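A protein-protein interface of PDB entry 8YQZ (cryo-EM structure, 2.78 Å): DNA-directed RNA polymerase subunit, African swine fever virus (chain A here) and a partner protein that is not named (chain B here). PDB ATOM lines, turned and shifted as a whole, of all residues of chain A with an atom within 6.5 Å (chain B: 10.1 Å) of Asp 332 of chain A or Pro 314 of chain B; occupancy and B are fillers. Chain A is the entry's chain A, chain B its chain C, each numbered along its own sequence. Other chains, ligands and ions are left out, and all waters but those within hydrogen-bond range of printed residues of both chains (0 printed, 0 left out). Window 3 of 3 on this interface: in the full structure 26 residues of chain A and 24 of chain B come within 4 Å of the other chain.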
ATOM      1  N   ASN A 330      -5.359 -10.569  11.763  1.00  0.00           N
ATOM      2  CA  ASN A 330      -6.256 -11.690  11.503  1.00  0.00           C
ATOM      3  C   ASN A 330      -5.527 -12.956  11.923  1.00  0.00           C
ATOM      4  O   ASN A 330      -4.582 -13.381  11.265  1.00  0.00           O
ATOM      5  CB  ASN A 330      -6.670 -11.729  10.035  1.00  0.00           C
ATOM      6  CG  ASN A 330      -7.748 -12.748   9.747  1.00  0.00           C
ATOM      7  OD1 ASN A 330      -7.940 -13.688  10.488  1.00  0.00           O
ATOM      8  ND2 ASN A 330      -8.471 -12.544   8.672  1.00  0.00           N
ATOM      9  N   SER A 331      -5.960 -13.551  13.025  1.00  0.00           N
ATOM     10  CA  SER A 331      -5.245 -14.680  13.593  1.00  0.00           C
ATOM     11  C   SER A 331      -5.595 -16.000  12.931  1.00  0.00           C
ATOM     12  O   SER A 331      -5.002 -17.017  13.277  1.00  0.00           O
ATOM     13  CB  SER A 331      -5.496 -14.747  15.099  1.00  0.00           C
ATOM     14  OG  SER A 331      -6.817 -15.117  15.392  1.00  0.00           O
ATOM     15  N   ASP A 332      -6.518 -16.008  11.985  1.00  0.00           N
ATOM     16  CA  ASP A 332      -6.827 -17.195  11.206  1.00  0.00           C
ATOM     17  C   ASP A 332      -6.017 -17.284   9.926  1.00  0.00           C
ATOM     18  O   ASP A 332      -6.219 -18.213   9.148  1.00  0.00           O
ATOM     19  CB  ASP A 332      -8.312 -17.225  10.873  1.00  0.00           C
ATOM     20  CG  ASP A 332      -9.156 -17.615  12.052  1.00  0.00           C
ATOM     21  OD1 ASP A 332      -8.836 -18.621  12.713  1.00  0.00           O
ATOM     22  OD2 ASP A 332     -10.132 -16.901  12.337  1.00  0.00           O
ATOM     23  N   LEU A 333      -5.113 -16.345   9.694  1.00  0.00           N
ATOM     24  CA  LEU A 333      -4.220 -16.381   8.554  1.00  0.00           C
ATOM     25  C   LEU A 333      -2.888 -16.997   8.947  1.00  0.00           C
ATOM     26  O   LEU A 333      -2.394 -16.774  10.051  1.00  0.00           O
ATOM     27  CB  LEU A 333      -3.989 -14.975   8.016  1.00  0.00           C
ATOM     28  CG  LEU A 333      -5.110 -14.262   7.286  1.00  0.00           C
ATOM     29  CD1 LEU A 333      -4.657 -12.882   6.954  1.00  0.00           C
ATOM     30  CD2 LEU A 333      -5.522 -15.004   6.053  1.00  0.00           C
ATOM     31  N   HIS A 334      -2.309 -17.772   8.039  1.00  0.00           N
ATOM     32  CA  HIS A 334      -0.957 -18.251   8.244  1.00  0.00           C
ATOM     33  C   HIS A 334       0.028 -17.096   8.130  1.00  0.00           C
ATOM     34  O   HIS A 334      -0.305 -16.004   7.687  1.00  0.00           O
ATOM     35  CB  HIS A 334      -0.608 -19.334   7.235  1.00  0.00           C
ATOM     36  CG  HIS A 334      -1.298 -20.631   7.484  1.00  0.00           C
ATOM     37  ND1 HIS A 334      -0.644 -21.743   7.958  1.00  0.00           N
ATOM     38  CD2 HIS A 334      -2.590 -20.990   7.343  1.00  0.00           C
ATOM     39  CE1 HIS A 334      -1.500 -22.737   8.081  1.00  0.00           C
ATOM     40  NE2 HIS A 334      -2.690 -22.305   7.716  1.00  0.00           N
ATOM     41  N   GLU A 337       0.539 -15.650   4.577  1.00  0.00           N
ATOM     42  CA  GLU A 337      -0.685 -15.336   3.874  1.00  0.00           C
ATOM     43  C   GLU A 337      -1.044 -13.885   4.133  1.00  0.00           C
ATOM     44  O   GLU A 337      -0.671 -13.310   5.154  1.00  0.00           O
ATOM     45  CB  GLU A 337      -1.818 -16.242   4.319  1.00  0.00           C
ATOM     46  CG  GLU A 337      -1.802 -17.598   3.688  1.00  0.00           C
ATOM     47  CD  GLU A 337      -2.835 -18.510   4.288  1.00  0.00           C
ATOM     48  OE1 GLU A 337      -3.391 -18.169   5.345  1.00  0.00           O
ATOM     49  OE2 GLU A 337      -3.106 -19.573   3.710  1.00  0.00           O
ATOM     50  N   ASN A 438     -16.142 -10.868   1.892  1.00  0.00           N
ATOM     51  CA  ASN A 438     -17.048  -9.924   2.535  1.00  0.00           C
ATOM     52  C   ASN A 438     -16.868  -8.557   1.894  1.00  0.00           C
ATOM     53  O   ASN A 438     -15.763  -8.009   1.936  1.00  0.00           O
ATOM     54  CB  ASN A 438     -16.759  -9.856   4.029  1.00  0.00           C
ATOM     55  CG  ASN A 438     -17.745  -8.985   4.784  1.00  0.00           C
ATOM     56  OD1 ASN A 438     -18.783  -8.608   4.260  1.00  0.00           O
ATOM     57  ND2 ASN A 438     -17.413  -8.656   6.020  1.00  0.00           N
ATOM     58  N   ASN A 447      -1.293 -12.045   9.732  1.00  0.00           N
ATOM     59  CA  ASN A 447      -1.038 -12.597  11.050  1.00  0.00           C
ATOM     60  C   ASN A 447      -0.112 -11.690  11.849  1.00  0.00           C
ATOM     61  O   ASN A 447       0.791 -11.055  11.310  1.00  0.00           O
ATOM     62  CB  ASN A 447      -0.452 -13.995  10.908  1.00  0.00           C
ATOM     63  CG  ASN A 447      -0.688 -14.851  12.112  1.00  0.00           C
ATOM     64  OD1 ASN A 447      -0.367 -14.472  13.220  1.00  0.00           O
ATOM     65  ND2 ASN A 447      -1.328 -15.979  11.911  1.00  0.00           N
ATOM     66  N   THR A 533      -8.732 -25.831  15.156  1.00  0.00           N
ATOM     67  CA  THR A 533      -8.414 -24.621  14.425  1.00  0.00           C
ATOM     68  C   THR A 533      -6.990 -24.609  13.881  1.00  0.00           C
ATOM     69  O   THR A 533      -6.701 -23.831  12.968  1.00  0.00           O
ATOM     70  CB  THR A 533      -8.683 -23.407  15.335  1.00  0.00           C
ATOM     71  OG1 THR A 533     -10.084 -23.115  15.321  1.00  0.00           O
ATOM     72  CG2 THR A 533      -7.960 -22.180  14.915  1.00  0.00           C
ATOM     73  N   GLN A 535      -5.365 -26.138  11.767  1.00  0.00           N
ATOM     74  CA  GLN A 535      -5.219 -26.367  10.332  1.00  0.00           C
ATOM     75  C   GLN A 535      -4.141 -27.388  10.012  1.00  0.00           C
ATOM     76  O   GLN A 535      -3.592 -27.392   8.913  1.00  0.00           O
ATOM     77  CB  GLN A 535      -4.965 -25.065   9.575  1.00  0.00           C
ATOM     78  CG  GLN A 535      -6.221 -24.513   8.943  1.00  0.00           C
ATOM     79  CD  GLN A 535      -6.210 -23.016   8.812  1.00  0.00           C
ATOM     80  OE1 GLN A 535      -5.389 -22.456   8.095  1.00  0.00           O
ATOM     81  NE2 GLN A 535      -7.134 -22.356   9.489  1.00  0.00           N
ATOM     82  N   PHE A 634       2.199 -20.960  13.707  1.00  0.00           N
ATOM     83  CA  PHE A 634       0.757 -20.839  13.562  1.00  0.00           C
ATOM     84  C   PHE A 634       0.017 -21.869  14.401  1.00  0.00           C
ATOM     85  O   PHE A 634      -0.986 -21.550  15.035  1.00  0.00           O
ATOM     86  CB  PHE A 634       0.378 -20.977  12.090  1.00  0.00           C
ATOM     87  CG  PHE A 634      -1.088 -20.936  11.840  1.00  0.00           C
ATOM     88  CD1 PHE A 634      -1.746 -19.739  11.746  1.00  0.00           C
ATOM     89  CD2 PHE A 634      -1.813 -22.098  11.716  1.00  0.00           C
ATOM     90  CE1 PHE A 634      -3.087 -19.703  11.534  1.00  0.00           C
ATOM     91  CE2 PHE A 634      -3.147 -22.056  11.507  1.00  0.00           C
ATOM     92  CZ  PHE A 634      -3.784 -20.859  11.411  1.00  0.00           C
ATOM     93  N   GLN A 637       0.211 -21.247  18.103  1.00  0.00           N
ATOM     94  CA  GLN A 637      -0.511 -20.023  18.408  1.00  0.00           C
ATOM     95  C   GLN A 637      -2.008 -20.265  18.504  1.00  0.00           C
ATOM     96  O   GLN A 637      -2.703 -19.581  19.256  1.00  0.00           O
ATOM     97  CB  GLN A 637      -0.187 -18.995  17.343  1.00  0.00           C
ATOM     98  CG  GLN A 637      -1.162 -17.907  17.195  1.00  0.00           C
ATOM     99  CD  GLN A 637      -0.734 -16.935  16.159  1.00  0.00           C
ATOM    100  OE1 GLN A 637       0.412 -16.933  15.737  1.00  0.00           O
ATOM    101  NE2 GLN A 637      -1.658 -16.113  15.714  1.00  0.00           N
ATOM    102  N   GLN A 638      -2.528 -21.223  17.746  1.00  0.00           N
ATOM    103  CA  GLN A 638      -3.935 -21.583  17.839  1.00  0.00           C
ATOM    104  C   GLN A 638      -4.220 -22.426  19.069  1.00  0.00           C
ATOM    105  O   GLN A 638      -5.298 -22.319  19.650  1.00  0.00           O
ATOM    106  CB  GLN A 638      -4.378 -22.327  16.576  1.00  0.00           C
ATOM    107  CG  GLN A 638      -4.134 -21.606  15.273  1.00  0.00           C
ATOM    108  CD  GLN A 638      -4.779 -20.245  15.219  1.00  0.00           C
ATOM    109  OE1 GLN A 638      -5.922 -20.078  15.598  1.00  0.00           O
ATOM    110  NE2 GLN A 638      -4.043 -19.264  14.745  1.00  0.00           N
ATOM    111  N   ARG B 171     -28.789 -11.150  12.735  1.00  0.00           N
ATOM    112  CA  ARG B 171     -27.412 -11.443  12.390  1.00  0.00           C
ATOM    113  C   ARG B 171     -26.942 -10.605  11.207  1.00  0.00           C
ATOM    114  O   ARG B 171     -25.747 -10.328  11.082  1.00  0.00           O
ATOM    115  CB  ARG B 171     -27.305 -12.932  12.088  1.00  0.00           C
ATOM    116  CG  ARG B 171     -25.938 -13.483  12.059  1.00  0.00           C
ATOM    117  CD  ARG B 171     -26.016 -14.982  12.131  1.00  0.00           C
ATOM    118  NE  ARG B 171     -26.835 -15.526  11.060  1.00  0.00           N
ATOM    119  CZ  ARG B 171     -26.368 -15.866   9.869  1.00  0.00           C
ATOM    120  NH1 ARG B 171     -25.090 -15.742   9.569  1.00  0.00           N
ATOM    121  NH2 ARG B 171     -27.206 -16.340   8.956  1.00  0.00           N
ATOM    122  N   LYS B 284     -22.419 -23.440   3.944  1.00  0.00           N
ATOM    123  CA  LYS B 284     -22.234 -22.014   3.761  1.00  0.00           C
ATOM    124  C   LYS B 284     -23.260 -21.231   4.563  1.00  0.00           C
ATOM    125  O   LYS B 284     -24.443 -21.577   4.591  1.00  0.00           O
ATOM    126  CB  LYS B 284     -22.337 -21.655   2.284  1.00  0.00           C
ATOM    127  CG  LYS B 284     -21.505 -20.461   1.894  1.00  0.00           C
ATOM    128  CD  LYS B 284     -20.085 -20.858   1.537  1.00  0.00           C
ATOM    129  CE  LYS B 284     -19.107 -19.740   1.859  1.00  0.00           C
ATOM    130  NZ  LYS B 284     -19.706 -18.402   1.627  1.00  0.00           N
ATOM    131  N   ASP B 285     -22.789 -20.169   5.217  1.00  0.00           N
ATOM    132  CA  ASP B 285     -23.612 -19.276   6.030  1.00  0.00           C
ATOM    133  C   ASP B 285     -24.204 -19.971   7.255  1.00  0.00           C
ATOM    134  O   ASP B 285     -25.300 -19.633   7.699  1.00  0.00           O
ATOM    135  CB  ASP B 285     -24.723 -18.634   5.198  1.00  0.00           C
ATOM    136  CG  ASP B 285     -24.909 -17.171   5.509  1.00  0.00           C
ATOM    137  OD1 ASP B 285     -23.996 -16.568   6.108  1.00  0.00           O
ATOM    138  OD2 ASP B 285     -25.975 -16.624   5.162  1.00  0.00           O
ATOM    139  N   GLU B 286     -23.490 -20.926   7.831  1.00  0.00           N
ATOM    140  CA  GLU B 286     -23.904 -21.492   9.101  1.00  0.00           C
ATOM    141  C   GLU B 286     -23.052 -20.927  10.232  1.00  0.00           C
ATOM    142  O   GLU B 286     -21.944 -20.432  10.026  1.00  0.00           O
ATOM    143  CB  GLU B 286     -23.816 -23.010   9.083  1.00  0.00           C
ATOM    144  CG  GLU B 286     -25.093 -23.699   8.681  1.00  0.00           C
ATOM    145  CD  GLU B 286     -26.235 -23.438   9.629  1.00  0.00           C
ATOM    146  OE1 GLU B 286     -25.982 -23.064  10.785  1.00  0.00           O
ATOM    147  OE2 GLU B 286     -27.394 -23.632   9.222  1.00  0.00           O
ATOM    148  N   THR B 287     -23.584 -21.008  11.444  1.00  0.00           N
ATOM    149  CA  THR B 287     -23.029 -20.293  12.578  1.00  0.00           C
ATOM    150  C   THR B 287     -22.627 -21.284  13.665  1.00  0.00           C
ATOM    151  O   THR B 287     -22.697 -22.496  13.484  1.00  0.00           O
ATOM    152  CB  THR B 287     -24.029 -19.253  13.104  1.00  0.00           C
ATOM    153  OG1 THR B 287     -25.281 -19.881  13.382  1.00  0.00           O
ATOM    154  CG2 THR B 287     -24.261 -18.193  12.070  1.00  0.00           C
ATOM    155  N   HIS B 288     -22.194 -20.747  14.803  1.00  0.00           N
ATOM    156  CA  HIS B 288     -21.733 -21.569  15.913  1.00  0.00           C
ATOM    157  C   HIS B 288     -22.849 -22.381  16.543  1.00  0.00           C
ATOM    158  O   HIS B 288     -22.567 -23.382  17.200  1.00  0.00           O
ATOM    159  CB  HIS B 288     -21.075 -20.695  16.982  1.00  0.00           C
ATOM    160  CG  HIS B 288     -19.755 -20.132  16.574  1.00  0.00           C
ATOM    161  ND1 HIS B 288     -18.588 -20.858  16.637  1.00  0.00           N
ATOM    162  CD2 HIS B 288     -19.413 -18.915  16.100  1.00  0.00           C
ATOM    163  CE1 HIS B 288     -17.584 -20.112  16.218  1.00  0.00           C
ATOM    164  NE2 HIS B 288     -18.058 -18.927  15.887  1.00  0.00           N
ATOM    165  N   TYR B 310     -15.279 -28.472  14.861  1.00  0.00           N
ATOM    166  CA  TYR B 310     -15.912 -27.595  13.891  1.00  0.00           C
ATOM    167  C   TYR B 310     -15.172 -26.272  13.863  1.00  0.00           C
ATOM    168  O   TYR B 310     -14.373 -25.965  14.744  1.00  0.00           O
ATOM    169  CB  TYR B 310     -17.405 -27.390  14.195  1.00  0.00           C
ATOM    170  CG  TYR B 310     -17.702 -26.352  15.246  1.00  0.00           C
ATOM    171  CD1 TYR B 310     -17.642 -26.670  16.584  1.00  0.00           C
ATOM    172  CD2 TYR B 310     -18.059 -25.062  14.900  1.00  0.00           C
ATOM    173  CE1 TYR B 310     -17.904 -25.744  17.536  1.00  0.00           C
ATOM    174  CE2 TYR B 310     -18.322 -24.130  15.850  1.00  0.00           C
ATOM    175  CZ  TYR B 310     -18.245 -24.474  17.172  1.00  0.00           C
ATOM    176  OH  TYR B 310     -18.513 -23.549  18.153  1.00  0.00           O
ATOM    177  N   GLN B 311     -15.439 -25.489  12.828  1.00  0.00           N
ATOM    178  CA  GLN B 311     -14.770 -24.214  12.650  1.00  0.00           C
ATOM    179  C   GLN B 311     -15.710 -23.239  11.969  1.00  0.00           C
ATOM    180  O   GLN B 311     -16.364 -23.598  10.992  1.00  0.00           O
ATOM    181  CB  GLN B 311     -13.503 -24.390  11.822  1.00  0.00           C
ATOM    182  CG  GLN B 311     -12.362 -23.539  12.261  1.00  0.00           C
ATOM    183  CD  GLN B 311     -11.161 -23.737  11.383  1.00  0.00           C
ATOM    184  OE1 GLN B 311     -11.067 -24.730  10.664  1.00  0.00           O
ATOM    185  NE2 GLN B 311     -10.235 -22.792  11.426  1.00  0.00           N
ATOM    186  N   CYS B 312     -15.790 -22.019  12.492  1.00  0.00           N
ATOM    187  CA  CYS B 312     -16.483 -20.913  11.835  1.00  0.00           C
ATOM    188  C   CYS B 312     -15.518 -19.738  11.787  1.00  0.00           C
ATOM    189  O   CYS B 312     -15.568 -18.848  12.635  1.00  0.00           O
ATOM    190  CB  CYS B 312     -17.779 -20.525  12.546  1.00  0.00           C
ATOM    191  SG  CYS B 312     -19.019 -21.793  12.695  1.00  0.00           S
ATOM    192  N   VAL B 313     -14.664 -19.721  10.779  1.00  0.00           N
ATOM    193  CA  VAL B 313     -13.718 -18.617  10.600  1.00  0.00           C
ATOM    194  C   VAL B 313     -14.479 -17.384  10.133  1.00  0.00           C
ATOM    195  O   VAL B 313     -15.234 -17.467   9.154  1.00  0.00           O
ATOM    196  CB  VAL B 313     -12.639 -19.008   9.599  1.00  0.00           C
ATOM    197  CG1 VAL B 313     -11.739 -17.855   9.330  1.00  0.00           C
ATOM    198  CG2 VAL B 313     -11.855 -20.180  10.123  1.00  0.00           C
ATOM    199  N   PRO B 314     -14.326 -16.232  10.791  1.00  0.00           N
ATOM    200  CA  PRO B 314     -15.169 -15.082  10.450  1.00  0.00           C
ATOM    201  C   PRO B 314     -15.058 -14.628   9.009  1.00  0.00           C
ATOM    202  O   PRO B 314     -16.051 -14.147   8.458  1.00  0.00           O
ATOM    203  CB  PRO B 314     -14.683 -14.006  11.424  1.00  0.00           C
ATOM    204  CG  PRO B 314     -14.147 -14.744  12.552  1.00  0.00           C
ATOM    205  CD  PRO B 314     -13.512 -15.963  11.984  1.00  0.00           C
ATOM    206  N   HIS B 315     -13.906 -14.779   8.369  1.00  0.00           N
ATOM    207  CA  HIS B 315     -13.720 -14.294   7.011  1.00  0.00           C
ATOM    208  C   HIS B 315     -14.075 -15.327   5.951  1.00  0.00           C
ATOM    209  O   HIS B 315     -13.856 -15.071   4.767  1.00  0.00           O
ATOM    210  CB  HIS B 315     -12.283 -13.796   6.805  1.00  0.00           C
ATOM    211  CG  HIS B 315     -11.241 -14.874   6.737  1.00  0.00           C
ATOM    212  ND1 HIS B 315     -11.051 -15.659   5.624  1.00  0.00           N
ATOM    213  CD2 HIS B 315     -10.299 -15.259   7.628  1.00  0.00           C
ATOM    214  CE1 HIS B 315     -10.059 -16.501   5.843  1.00  0.00           C
ATOM    215  NE2 HIS B 315      -9.585 -16.278   7.051  1.00  0.00           N
ATOM    216  N   LYS B 316     -14.630 -16.470   6.331  1.00  0.00           N
ATOM    217  CA  LYS B 316     -15.014 -17.481   5.363  1.00  0.00           C
ATOM    218  C   LYS B 316     -16.512 -17.655   5.207  1.00  0.00           C
ATOM    219  O   LYS B 316     -16.942 -18.167   4.170  1.00  0.00           O
ATOM    220  CB  LYS B 316     -14.393 -18.833   5.723  1.00  0.00           C
ATOM    221  CG  LYS B 316     -12.902 -18.784   5.788  1.00  0.00           C
ATOM    222  CD  LYS B 316     -12.291 -20.105   5.447  1.00  0.00           C
ATOM    223  CE  LYS B 316     -12.363 -20.318   3.958  1.00  0.00           C
ATOM    224  NZ  LYS B 316     -11.806 -19.159   3.226  1.00  0.00           N
ATOM    225  N   GLN B 317     -17.312 -17.244   6.188  1.00  0.00           N
ATOM    226  CA  GLN B 317     -18.769 -17.308   6.116  1.00  0.00           C
ATOM    227  C   GLN B 317     -19.268 -18.725   5.847  1.00  0.00           C
ATOM    228  O   GLN B 317     -20.153 -18.946   5.022  1.00  0.00           O
ATOM    229  CB  GLN B 317     -19.305 -16.338   5.068  1.00  0.00           C
ATOM    230  CG  GLN B 317     -19.255 -14.883   5.482  1.00  0.00           C
ATOM    231  CD  GLN B 317     -18.703 -13.983   4.402  1.00  0.00           C
ATOM    232  OE1 GLN B 317     -17.611 -14.204   3.894  1.00  0.00           O
ATOM    233  NE2 GLN B 317     -19.458 -12.958   4.048  1.00  0.00           N
ATOM    234  N   GLU B 318     -18.703 -19.694   6.559  1.00  0.00           N
ATOM    235  CA  GLU B 318     -19.129 -21.079   6.437  1.00  0.00           C
ATOM    236  C   GLU B 318     -18.758 -21.817   7.711  1.00  0.00           C
ATOM    237  O   GLU B 318     -17.937 -21.351   8.499  1.00  0.00           O
ATOM    238  CB  GLU B 318     -18.495 -21.752   5.223  1.00  0.00           C
ATOM    239  CG  GLU B 318     -17.122 -22.292   5.472  1.00  0.00           C
ATOM    240  CD  GLU B 318     -16.224 -22.154   4.275  1.00  0.00           C
ATOM    241  OE1 GLU B 318     -16.634 -21.496   3.301  1.00  0.00           O
ATOM    242  OE2 GLU B 318     -15.107 -22.700   4.303  1.00  0.00           O
ATOM    243  N   MET B 319     -19.379 -22.974   7.902  1.00  0.00           N
ATOM    244  CA  MET B 319     -19.087 -23.862   9.016  1.00  0.00           C
ATOM    245  C   MET B 319     -18.556 -25.175   8.464  1.00  0.00           C
ATOM    246  O   MET B 319     -19.186 -25.780   7.596  1.00  0.00           O
ATOM    247  CB  MET B 319     -20.342 -24.106   9.854  1.00  0.00           C
ATOM    248  CG  MET B 319     -20.111 -24.788  11.191  1.00  0.00           C
ATOM    249  SD  MET B 319     -20.093 -26.589  11.157  1.00  0.00           S
ATOM    250  CE  MET B 319     -21.709 -26.959  10.514  1.00  0.00           C
ATOM    251  N   VAL B 320     -17.406 -25.615   8.963  1.00  0.00           N
ATOM    252  CA  VAL B 320     -16.768 -26.851   8.524  1.00  0.00           C
ATOM    253  C   VAL B 320     -16.701 -27.802   9.707  1.00  0.00           C
ATOM    254  O   VAL B 320     -16.065 -27.494  10.716  1.00  0.00           O
ATOM    255  CB  VAL B 320     -15.361 -26.600   7.964  1.00  0.00           C
ATOM    256  CG1 VAL B 320     -14.780 -27.880   7.412  1.00  0.00           C
ATOM    257  CG2 VAL B 320     -15.389 -25.531   6.912  1.00  0.00           C
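Of the 13 printed residues of chain A, 4 touch a printed residue of chain B.
Of the 17 printed residues of chain B, 4 touch a printed residue of chain A.
Hydrophobic or aromatic side chains of chain B within 4 Å of the printed part of chain A: Val 313, Pro 314 and His 315.
Among the printed residues, 5 pairs touch across the chains.
Among the printed residues, no Asp or Glu carboxylate lies within 4 Å of a Lys or Arg side-chain nitrogen of the other chain.
Of the printed residues of chain B, Asn 330 of chain A touches His 315.
Ser 331 of chain A touches none of the printed residues of chain B.
Asp 332 of chain A touches just these residues of chain B: Val 313 and Pro 314.
No residue of chain B comes within 4 Å of Leu 333 of chain A.
Asn 438 of chain A touches none of the printed residues of chain B.
Printed residues of chain B within 4 Å of Thr 533 of chain A: Gln 311 (3.8 Å).
Of the printed residues of chain A, Gln 311 of chain B touches Thr 533 and Gln 535.
Glu 318 of chain B touches none of the printed residues of chain A.
The nearest residue of chain B that does not touch Asp 332 of chain A is His 315 of chain B (4.1 Å).
The nearest printed residue of chain B that does not touch Thr 533 of chain A is Tyr 310 of chain B (5.2 Å).
Among the printed residues, merely in contact across the chains: Asn 330 of chain A with His 315 of chain B (3.4 Å), Asp 332 of chain A with Val 313 of chain B (3.5 Å), Asp 332 of chain A with Pro 314 of chain B (3.5 Å), Thr 533 of chain A with Gln 311 of chain B (3.8 Å) and Gln 535 of chain A with Gln 311 of chain B (3.7 Å).
The side-chain amide oxygen of Asn 330 of chain A lies within hydrogen-bond range of the backbone NH of Asp 332 of chain A, 3.1 Å away.
NE2 of His 334 of chain A lies within hydrogen-bond range of OE1 of Gln 535 of chain A.
The backbone NH of Gln 311 of chain B sits at hydrogen-bond distance from the backbone carbonyl oxygen of Val 320 of chain B.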
